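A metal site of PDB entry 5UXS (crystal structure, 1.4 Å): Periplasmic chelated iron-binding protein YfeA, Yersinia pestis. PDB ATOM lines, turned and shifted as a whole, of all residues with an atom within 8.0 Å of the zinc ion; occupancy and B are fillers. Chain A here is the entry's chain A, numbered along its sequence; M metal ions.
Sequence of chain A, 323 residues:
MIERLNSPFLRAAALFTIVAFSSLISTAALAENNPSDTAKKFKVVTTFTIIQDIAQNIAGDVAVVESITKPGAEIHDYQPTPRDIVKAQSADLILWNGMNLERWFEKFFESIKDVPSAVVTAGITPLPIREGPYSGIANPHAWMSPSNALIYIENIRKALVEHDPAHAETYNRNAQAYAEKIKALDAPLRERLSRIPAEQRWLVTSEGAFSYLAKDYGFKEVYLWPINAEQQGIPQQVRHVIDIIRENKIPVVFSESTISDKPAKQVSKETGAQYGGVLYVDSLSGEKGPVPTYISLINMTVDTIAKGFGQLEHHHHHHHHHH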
ATOM      1  N   PHE A  48     -15.266  13.682  -5.423  1.00  0.00           N
ATOM      2  CA  PHE A  48     -14.815  13.578  -4.035  1.00  0.00           C
ATOM      3  C   PHE A  48     -14.446  12.135  -3.700  1.00  0.00           C
ATOM      4  O   PHE A  48     -14.594  11.223  -4.519  1.00  0.00           O
ATOM      5  CB  PHE A  48     -15.773  14.269  -3.035  1.00  0.00           C
ATOM      6  CG  PHE A  48     -17.041  13.485  -2.687  1.00  0.00           C
ATOM      7  CD1 PHE A  48     -18.010  13.235  -3.646  1.00  0.00           C
ATOM      8  CD2 PHE A  48     -17.243  13.028  -1.384  1.00  0.00           C
ATOM      9  CE1 PHE A  48     -19.184  12.546  -3.316  1.00  0.00           C
ATOM     10  CE2 PHE A  48     -18.426  12.340  -1.043  1.00  0.00           C
ATOM     11  CZ  PHE A  48     -19.377  12.089  -2.015  1.00  0.00           C
ATOM     12  N   GLU A  74     -12.999  20.401   2.293  1.00  0.00           N
ATOM     13  CA  GLU A  74     -14.435  20.659   2.306  1.00  0.00           C
ATOM     14  C   GLU A  74     -14.984  20.577   0.881  1.00  0.00           C
ATOM     15  O   GLU A  74     -14.500  21.281  -0.011  1.00  0.00           O
ATOM     16  CB  GLU A  74     -14.671  22.030   2.927  1.00  0.00           C
ATOM     17  CG  GLU A  74     -16.051  22.230   3.515  1.00  0.00           C
ATOM     18  CD  GLU A  74     -17.127  22.231   2.456  1.00  0.00           C
ATOM     19  OE1 GLU A  74     -17.106  23.116   1.567  1.00  0.00           O
ATOM     20  OE2 GLU A  74     -17.998  21.325   2.504  1.00  0.00           O
ATOM     21  N   ILE A  75     -15.997  19.744   0.681  1.00  0.00           N
ATOM     22  CA  ILE A  75     -16.442  19.387  -0.671  1.00  0.00           C
ATOM     23  C   ILE A  75     -17.609  20.197  -1.198  1.00  0.00           C
ATOM     24  O   ILE A  75     -17.821  20.232  -2.423  1.00  0.00           O
ATOM     25  CB  ILE A  75     -16.772  17.876  -0.781  1.00  0.00           C
ATOM     26  CG1 ILE A  75     -18.011  17.536   0.052  1.00  0.00           C
ATOM     27  CG2 ILE A  75     -15.569  17.042  -0.357  1.00  0.00           C
ATOM     28  CD1 ILE A  75     -18.383  16.063   0.014  1.00  0.00           C
ATOM     29  N   HIS A  76     -18.410  20.818  -0.322  1.00  0.00           N
ATOM     30  CA  HIS A  76     -19.633  21.459  -0.802  1.00  0.00           C
ATOM     31  C   HIS A  76     -19.316  22.732  -1.551  1.00  0.00           C
ATOM     32  O   HIS A  76     -19.843  22.988  -2.647  1.00  0.00           O
ATOM     33  CB  HIS A  76     -20.546  21.798   0.394  1.00  0.00           C
ATOM     34  CG  HIS A  76     -21.105  20.603   1.102  1.00  0.00           C
ATOM     35  ND1 HIS A  76     -22.446  20.243   1.021  1.00  0.00           N
ATOM     36  CD2 HIS A  76     -20.534  19.711   1.951  1.00  0.00           C
ATOM     37  CE1 HIS A  76     -22.651  19.180   1.771  1.00  0.00           C
ATOM     38  NE2 HIS A  76     -21.517  18.835   2.358  1.00  0.00           N
ATOM     39  N   LEU A 101     -24.915  18.428  -3.837  1.00  0.00           N
ATOM     40  CA  LEU A 101     -23.676  18.331  -3.071  1.00  0.00           C
ATOM     41  C   LEU A 101     -22.621  19.320  -3.569  1.00  0.00           C
ATOM     42  O   LEU A 101     -22.225  20.232  -2.856  1.00  0.00           O
ATOM     43  CB  LEU A 101     -23.121  16.900  -3.123  1.00  0.00           C
ATOM     44  CG  LEU A 101     -21.805  16.729  -2.345  1.00  0.00           C
ATOM     45  CD1 LEU A 101     -22.018  16.934  -0.835  1.00  0.00           C
ATOM     46  CD2 LEU A 101     -21.206  15.378  -2.621  1.00  0.00           C
ATOM     47  N   ASN A 139     -31.140  16.556   0.659  1.00  0.00           N
ATOM     48  CA  ASN A 139     -29.906  16.390   1.436  1.00  0.00           C
ATOM     49  C   ASN A 139     -28.964  15.513   0.614  1.00  0.00           C
ATOM     50  O   ASN A 139     -29.348  14.415   0.197  1.00  0.00           O
ATOM     51  CB  ASN A 139     -30.266  15.734   2.774  1.00  0.00           C
ATOM     52  CG  ASN A 139     -29.089  15.601   3.718  1.00  0.00           C
ATOM     53  OD1 ASN A 139     -27.976  15.294   3.277  1.00  0.00           O
ATOM     54  ND2 ASN A 139     -29.316  15.798   4.995  1.00  0.00           N
ATOM     55  N   PRO A 140     -27.741  15.959   0.328  1.00  0.00           N
ATOM     56  CA  PRO A 140     -26.891  15.190  -0.602  1.00  0.00           C
ATOM     57  C   PRO A 140     -26.251  13.948  -0.011  1.00  0.00           C
ATOM     58  O   PRO A 140     -25.779  13.108  -0.785  1.00  0.00           O
ATOM     59  CB  PRO A 140     -25.802  16.199  -0.995  1.00  0.00           C
ATOM     60  CG  PRO A 140     -25.695  17.099   0.221  1.00  0.00           C
ATOM     61  CD  PRO A 140     -27.128  17.250   0.712  1.00  0.00           C
ATOM     62  N   HIS A 141     -26.232  13.794   1.312  1.00  0.00           N
ATOM     63  CA  HIS A 141     -25.362  12.822   1.969  1.00  0.00           C
ATOM     64  C   HIS A 141     -25.946  11.398   1.951  1.00  0.00           C
ATOM     65  O   HIS A 141     -25.906  10.689   2.966  1.00  0.00           O
ATOM     66  CB  HIS A 141     -25.051  13.253   3.398  1.00  0.00           C
ATOM     67  CG  HIS A 141     -24.447  14.616   3.535  1.00  0.00           C
ATOM     68  ND1 HIS A 141     -25.192  15.749   3.776  1.00  0.00           N
ATOM     69  CD2 HIS A 141     -23.147  15.034   3.489  1.00  0.00           C
ATOM     70  CE1 HIS A 141     -24.395  16.797   3.888  1.00  0.00           C
ATOM     71  NE2 HIS A 141     -23.144  16.392   3.731  1.00  0.00           N
ATOM     72  N   TRP A 143     -24.962   8.586   0.742  1.00  0.00           N
ATOM     73  CA  TRP A 143     -24.047   7.456   0.897  1.00  0.00           C
ATOM     74  C   TRP A 143     -23.894   6.996   2.345  1.00  0.00           C
ATOM     75  O   TRP A 143     -23.277   5.958   2.567  1.00  0.00           O
ATOM     76  CB  TRP A 143     -22.668   7.819   0.338  1.00  0.00           C
ATOM     77  CG  TRP A 143     -21.987   8.956   1.065  1.00  0.00           C
ATOM     78  CD1 TRP A 143     -21.203   8.872   2.178  1.00  0.00           C
ATOM     79  CD2 TRP A 143     -22.061  10.348   0.729  1.00  0.00           C
ATOM     80  NE1 TRP A 143     -20.780  10.130   2.563  1.00  0.00           N
ATOM     81  CE2 TRP A 143     -21.296  11.050   1.681  1.00  0.00           C
ATOM     82  CE3 TRP A 143     -22.708  11.066  -0.285  1.00  0.00           C
ATOM     83  CZ2 TRP A 143     -21.152  12.446   1.652  1.00  0.00           C
ATOM     84  CZ3 TRP A 143     -22.564  12.452  -0.313  1.00  0.00           C
ATOM     85  CH2 TRP A 143     -21.777  13.125   0.642  1.00  0.00           C
ATOM     86  N   GLU A 207     -22.469  19.528  11.053  1.00  0.00           N
ATOM     87  CA  GLU A 207     -23.311  19.514   9.862  1.00  0.00           C
ATOM     88  C   GLU A 207     -24.389  18.452  10.037  1.00  0.00           C
ATOM     89  O   GLU A 207     -24.137  17.380  10.591  1.00  0.00           O
ATOM     90  CB  GLU A 207     -22.486  19.181   8.616  1.00  0.00           C
ATOM     91  CG  GLU A 207     -23.303  19.386   7.323  1.00  0.00           C
ATOM     92  CD  GLU A 207     -22.604  18.975   6.026  1.00  0.00           C
ATOM     93  OE1 GLU A 207     -21.634  18.172   6.037  1.00  0.00           O
ATOM     94  OE2 GLU A 207     -23.064  19.466   4.974  1.00  0.00           O
ATOM     95  N   GLY A 208     -25.589  18.756   9.538  1.00  0.00           N
ATOM     96  CA  GLY A 208     -26.678  17.785   9.464  1.00  0.00           C
ATOM     97  C   GLY A 208     -26.493  16.778   8.338  1.00  0.00           C
ATOM     98  O   GLY A 208     -27.377  16.593   7.499  1.00  0.00           O
ATOM     99  N   ALA A 209     -25.331  16.126   8.327  1.00  0.00           N
ATOM    100  CA  ALA A 209     -24.906  15.272   7.235  1.00  0.00           C
ATOM    101  C   ALA A 209     -25.297  13.823   7.420  1.00  0.00           C
ATOM    102  O   ALA A 209     -24.981  12.997   6.553  1.00  0.00           O
ATOM    103  CB  ALA A 209     -23.381  15.357   7.101  1.00  0.00           C
ATOM    104  N   PHE A 210     -25.993  13.490   8.504  1.00  0.00           N
ATOM    105  CA  PHE A 210     -26.208  12.092   8.872  1.00  0.00           C
ATOM    106  C   PHE A 210     -27.663  11.678   8.755  1.00  0.00           C
ATOM    107  O   PHE A 210     -28.030  10.600   9.222  1.00  0.00           O
ATOM    108  CB  PHE A 210     -25.647  11.835  10.270  1.00  0.00           C
ATOM    109  CG  PHE A 210     -24.191  12.123  10.357  1.00  0.00           C
ATOM    110  CD1 PHE A 210     -23.268  11.145   9.994  1.00  0.00           C
ATOM    111  CD2 PHE A 210     -23.735  13.384  10.686  1.00  0.00           C
ATOM    112  CE1 PHE A 210     -21.903  11.414  10.005  1.00  0.00           C
ATOM    113  CE2 PHE A 210     -22.380  13.664  10.706  1.00  0.00           C
ATOM    114  CZ  PHE A 210     -21.465  12.677  10.356  1.00  0.00           C
ATOM    115  N   TRP A 225     -25.669  23.071  12.017  1.00  0.00           N
ATOM    116  CA  TRP A 225     -26.065  23.728  10.764  1.00  0.00           C
ATOM    117  C   TRP A 225     -26.573  22.666   9.795  1.00  0.00           C
ATOM    118  O   TRP A 225     -26.048  21.543   9.778  1.00  0.00           O
ATOM    119  CB  TRP A 225     -24.967  24.572  10.101  1.00  0.00           C
ATOM    120  CG  TRP A 225     -23.666  23.882   9.852  1.00  0.00           C
ATOM    121  CD1 TRP A 225     -23.296  23.210   8.716  1.00  0.00           C
ATOM    122  CD2 TRP A 225     -22.541  23.807  10.742  1.00  0.00           C
ATOM    123  NE1 TRP A 225     -22.010  22.731   8.843  1.00  0.00           N
ATOM    124  CE2 TRP A 225     -21.531  23.072  10.081  1.00  0.00           C
ATOM    125  CE3 TRP A 225     -22.294  24.292  12.028  1.00  0.00           C
ATOM    126  CZ2 TRP A 225     -20.280  22.816  10.666  1.00  0.00           C
ATOM    127  CZ3 TRP A 225     -21.052  24.025  12.617  1.00  0.00           C
ATOM    128  CH2 TRP A 225     -20.067  23.294  11.928  1.00  0.00           C
ATOM    129  N   PRO A 226     -27.604  22.965   8.997  1.00  0.00           N
ATOM    130  CA  PRO A 226     -28.228  21.892   8.200  1.00  0.00           C
ATOM    131  C   PRO A 226     -27.355  21.360   7.083  1.00  0.00           C
ATOM    132  O   PRO A 226     -27.370  20.148   6.808  1.00  0.00           O
ATOM    133  CB  PRO A 226     -29.526  22.533   7.689  1.00  0.00           C
ATOM    134  CG  PRO A 226     -29.299  24.002   7.769  1.00  0.00           C
ATOM    135  CD  PRO A 226     -28.316  24.248   8.891  1.00  0.00           C
ATOM    136  N   ILE A 227     -26.593  22.220   6.413  1.00  0.00           N
ATOM    137  CA  ILE A 227     -25.686  21.800   5.355  1.00  0.00           C
ATOM    138  C   ILE A 227     -24.545  22.807   5.314  1.00  0.00           C
ATOM    139  O   ILE A 227     -24.720  23.997   5.598  1.00  0.00           O
ATOM    140  CB  ILE A 227     -26.416  21.666   3.995  1.00  0.00           C
ATOM    141  CG1 ILE A 227     -25.489  21.110   2.895  1.00  0.00           C
ATOM    142  CG2 ILE A 227     -27.018  22.985   3.549  1.00  0.00           C
ATOM    143  CD1 ILE A 227     -26.237  20.636   1.646  1.00  0.00           C
ATOM    144  N   ASN A 228     -23.358  22.318   4.975  1.00  0.00           N
ATOM    145  CA  ASN A 228     -22.197  23.198   4.891  1.00  0.00           C
ATOM    146  C   ASN A 228     -22.482  24.345   3.929  1.00  0.00           C
ATOM    147  O   ASN A 228     -22.951  24.123   2.803  1.00  0.00           O
ATOM    148  CB  ASN A 228     -20.966  22.416   4.412  1.00  0.00           C
ATOM    149  CG  ASN A 228     -20.404  21.475   5.464  1.00  0.00           C
ATOM    150  OD1 ASN A 228     -20.885  21.426   6.583  1.00  0.00           O
ATOM    151  ND2 ASN A 228     -19.391  20.715   5.093  1.00  0.00           N
ATOM    152  N   GLN A 232     -21.838  28.591  10.075  1.00  0.00           N
ATOM    153  CA  GLN A 232     -21.553  27.301  10.713  1.00  0.00           C
ATOM    154  C   GLN A 232     -21.089  27.532  12.155  1.00  0.00           C
ATOM    155  O   GLN A 232     -19.897  27.716  12.409  1.00  0.00           O
ATOM    156  CB  GLN A 232     -20.524  26.534   9.901  1.00  0.00           C
ATOM    157  CG  GLN A 232     -21.012  26.139   8.520  1.00  0.00           C
ATOM    158  CD  GLN A 232     -19.963  25.404   7.710  1.00  0.00           C
ATOM    159  OE1 GLN A 232     -20.205  25.033   6.568  1.00  0.00           O
ATOM    160  NE2 GLN A 232     -18.794  25.183   8.301  1.00  0.00           N
ATOM    161  N   GLU A 256     -17.218  16.671  12.493  1.00  0.00           N
ATOM    162  CA  GLU A 256     -16.914  15.903  11.290  1.00  0.00           C
ATOM    163  C   GLU A 256     -15.575  16.326  10.685  1.00  0.00           C
ATOM    164  O   GLU A 256     -15.085  17.434  10.932  1.00  0.00           O
ATOM    165  CB  GLU A 256     -18.036  16.022  10.228  1.00  0.00           C
ATOM    166  CG  GLU A 256     -19.418  15.623  10.753  1.00  0.00           C
ATOM    167  CD  GLU A 256     -20.150  16.787  11.376  1.00  0.00           C
ATOM    168  OE1 GLU A 256     -20.236  17.842  10.709  1.00  0.00           O
ATOM    169  OE2 GLU A 256     -20.600  16.667  12.543  1.00  0.00           O
ATOM    170  N   THR A 258     -14.140  17.311   7.884  1.00  0.00           N
ATOM    171  CA  THR A 258     -13.764  18.415   7.001  1.00  0.00           C
ATOM    172  C   THR A 258     -14.143  19.784   7.540  1.00  0.00           C
ATOM    173  O   THR A 258     -13.916  20.786   6.849  1.00  0.00           O
ATOM    174  CB  THR A 258     -14.368  18.272   5.594  1.00  0.00           C
ATOM    175  OG1 THR A 258     -15.792  18.470   5.677  1.00  0.00           O
ATOM    176  CG2 THR A 258     -14.068  16.910   5.004  1.00  0.00           C
ATOM    177  N   ILE A 259     -14.721  19.871   8.732  1.00  0.00           N
ATOM    178  CA  ILE A 259     -15.174  21.146   9.286  1.00  0.00           C
ATOM    179  C   ILE A 259     -14.554  21.328  10.674  1.00  0.00           C
ATOM    180  O   ILE A 259     -13.880  20.453  11.199  1.00  0.00           O
ATOM    181  CB  ILE A 259     -16.719  21.270   9.275  1.00  0.00           C
ATOM    182  CG1 ILE A 259     -17.397  20.058   9.931  1.00  0.00           C
ATOM    183  CG2 ILE A 259     -17.211  21.423   7.834  1.00  0.00           C
ATOM    184  CD1 ILE A 259     -17.365  20.059  11.462  1.00  0.00           C
ATOM    185  N   VAL A 281     -17.782  11.661   7.068  1.00  0.00           N
ATOM    186  CA  VAL A 281     -18.917  11.672   6.159  1.00  0.00           C
ATOM    187  C   VAL A 281     -18.538  12.231   4.784  1.00  0.00           C
ATOM    188  O   VAL A 281     -18.781  11.583   3.750  1.00  0.00           O
ATOM    189  CB  VAL A 281     -20.149  12.390   6.752  1.00  0.00           C
ATOM    190  CG1 VAL A 281     -19.805  13.773   7.321  1.00  0.00           C
ATOM    191  CG2 VAL A 281     -21.271  12.509   5.690  1.00  0.00           C
ATOM    192  N   ASP A 282     -17.939  13.415   4.758  1.00  0.00           N
ATOM    193  CA  ASP A 282     -17.669  14.097   3.500  1.00  0.00           C
ATOM    194  C   ASP A 282     -16.324  13.720   2.896  1.00  0.00           C
ATOM    195  O   ASP A 282     -16.085  14.049   1.733  1.00  0.00           O
ATOM    196  CB  ASP A 282     -17.774  15.620   3.678  1.00  0.00           C
ATOM    197  CG  ASP A 282     -19.231  16.112   3.767  1.00  0.00           C
ATOM    198  OD1 ASP A 282     -20.144  15.295   3.561  1.00  0.00           O
ATOM    199  OD2 ASP A 282     -19.431  17.315   4.023  1.00  0.00           O
ATOM    200  N   SER A 283     -15.454  13.025   3.639  1.00  0.00           N
ATOM    201  CA  SER A 283     -14.162  12.653   3.092  1.00  0.00           C
ATOM    202  C   SER A 283     -13.635  11.423   3.809  1.00  0.00           C
ATOM    203  O   SER A 283     -13.876  11.220   5.003  1.00  0.00           O
ATOM    204  CB  SER A 283     -13.162  13.812   3.240  1.00  0.00           C
ATOM    205  OG  SER A 283     -11.895  13.484   2.668  1.00  0.00           O
HETATM  206 ZN    ZN M   1     -21.427  17.582   4.019  1.00  0.00          ZN
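The backbone NH of Glu 207 sits at hydrogen-bond distance from the side-chain carboxylate of Glu 256 (2.8 Å).
The side-chain carboxylate of Glu 74 sits at hydrogen-bond distance from the side-chain amide nitrogen of Asn 228, at 3.0 Å.
The side-chain carboxylate of Glu 74 lies within hydrogen-bond range of the backbone NH of His 76, 2.9 Å away.
The side-chain carboxylate of Glu 207 lies within hydrogen-bond range of the backbone NH of Asn 228, at 2.9 Å.
The side-chain amide oxygen (OD1) of Asn 228 lies within hydrogen-bond range of the indole nitrogen (NE1) of Trp 225.
A ring nitrogen (ND1) of His 141 is in hydrogen-bond range of the side-chain amide oxygen (OD1) of Asn 139 (2.9 Å).
ND2 of Asn 228 touches the zinc ion, 3.9 Å away.
Five residues have an atom within 4 Å of the zinc ion: His 76, His 141, Glu 207, Asn 228 and Asp 282.
The zinc ion is bound by OD2 of Asp 282, NE2 of His 76, NE2 of His 141 and OE1 of Glu 207.
Slightly farther from the zinc ion lies OD1 of Asp 282 (2.7 Å).
Slightly farther from the zinc ion lies OE2 of Glu 207 (2.7 Å).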
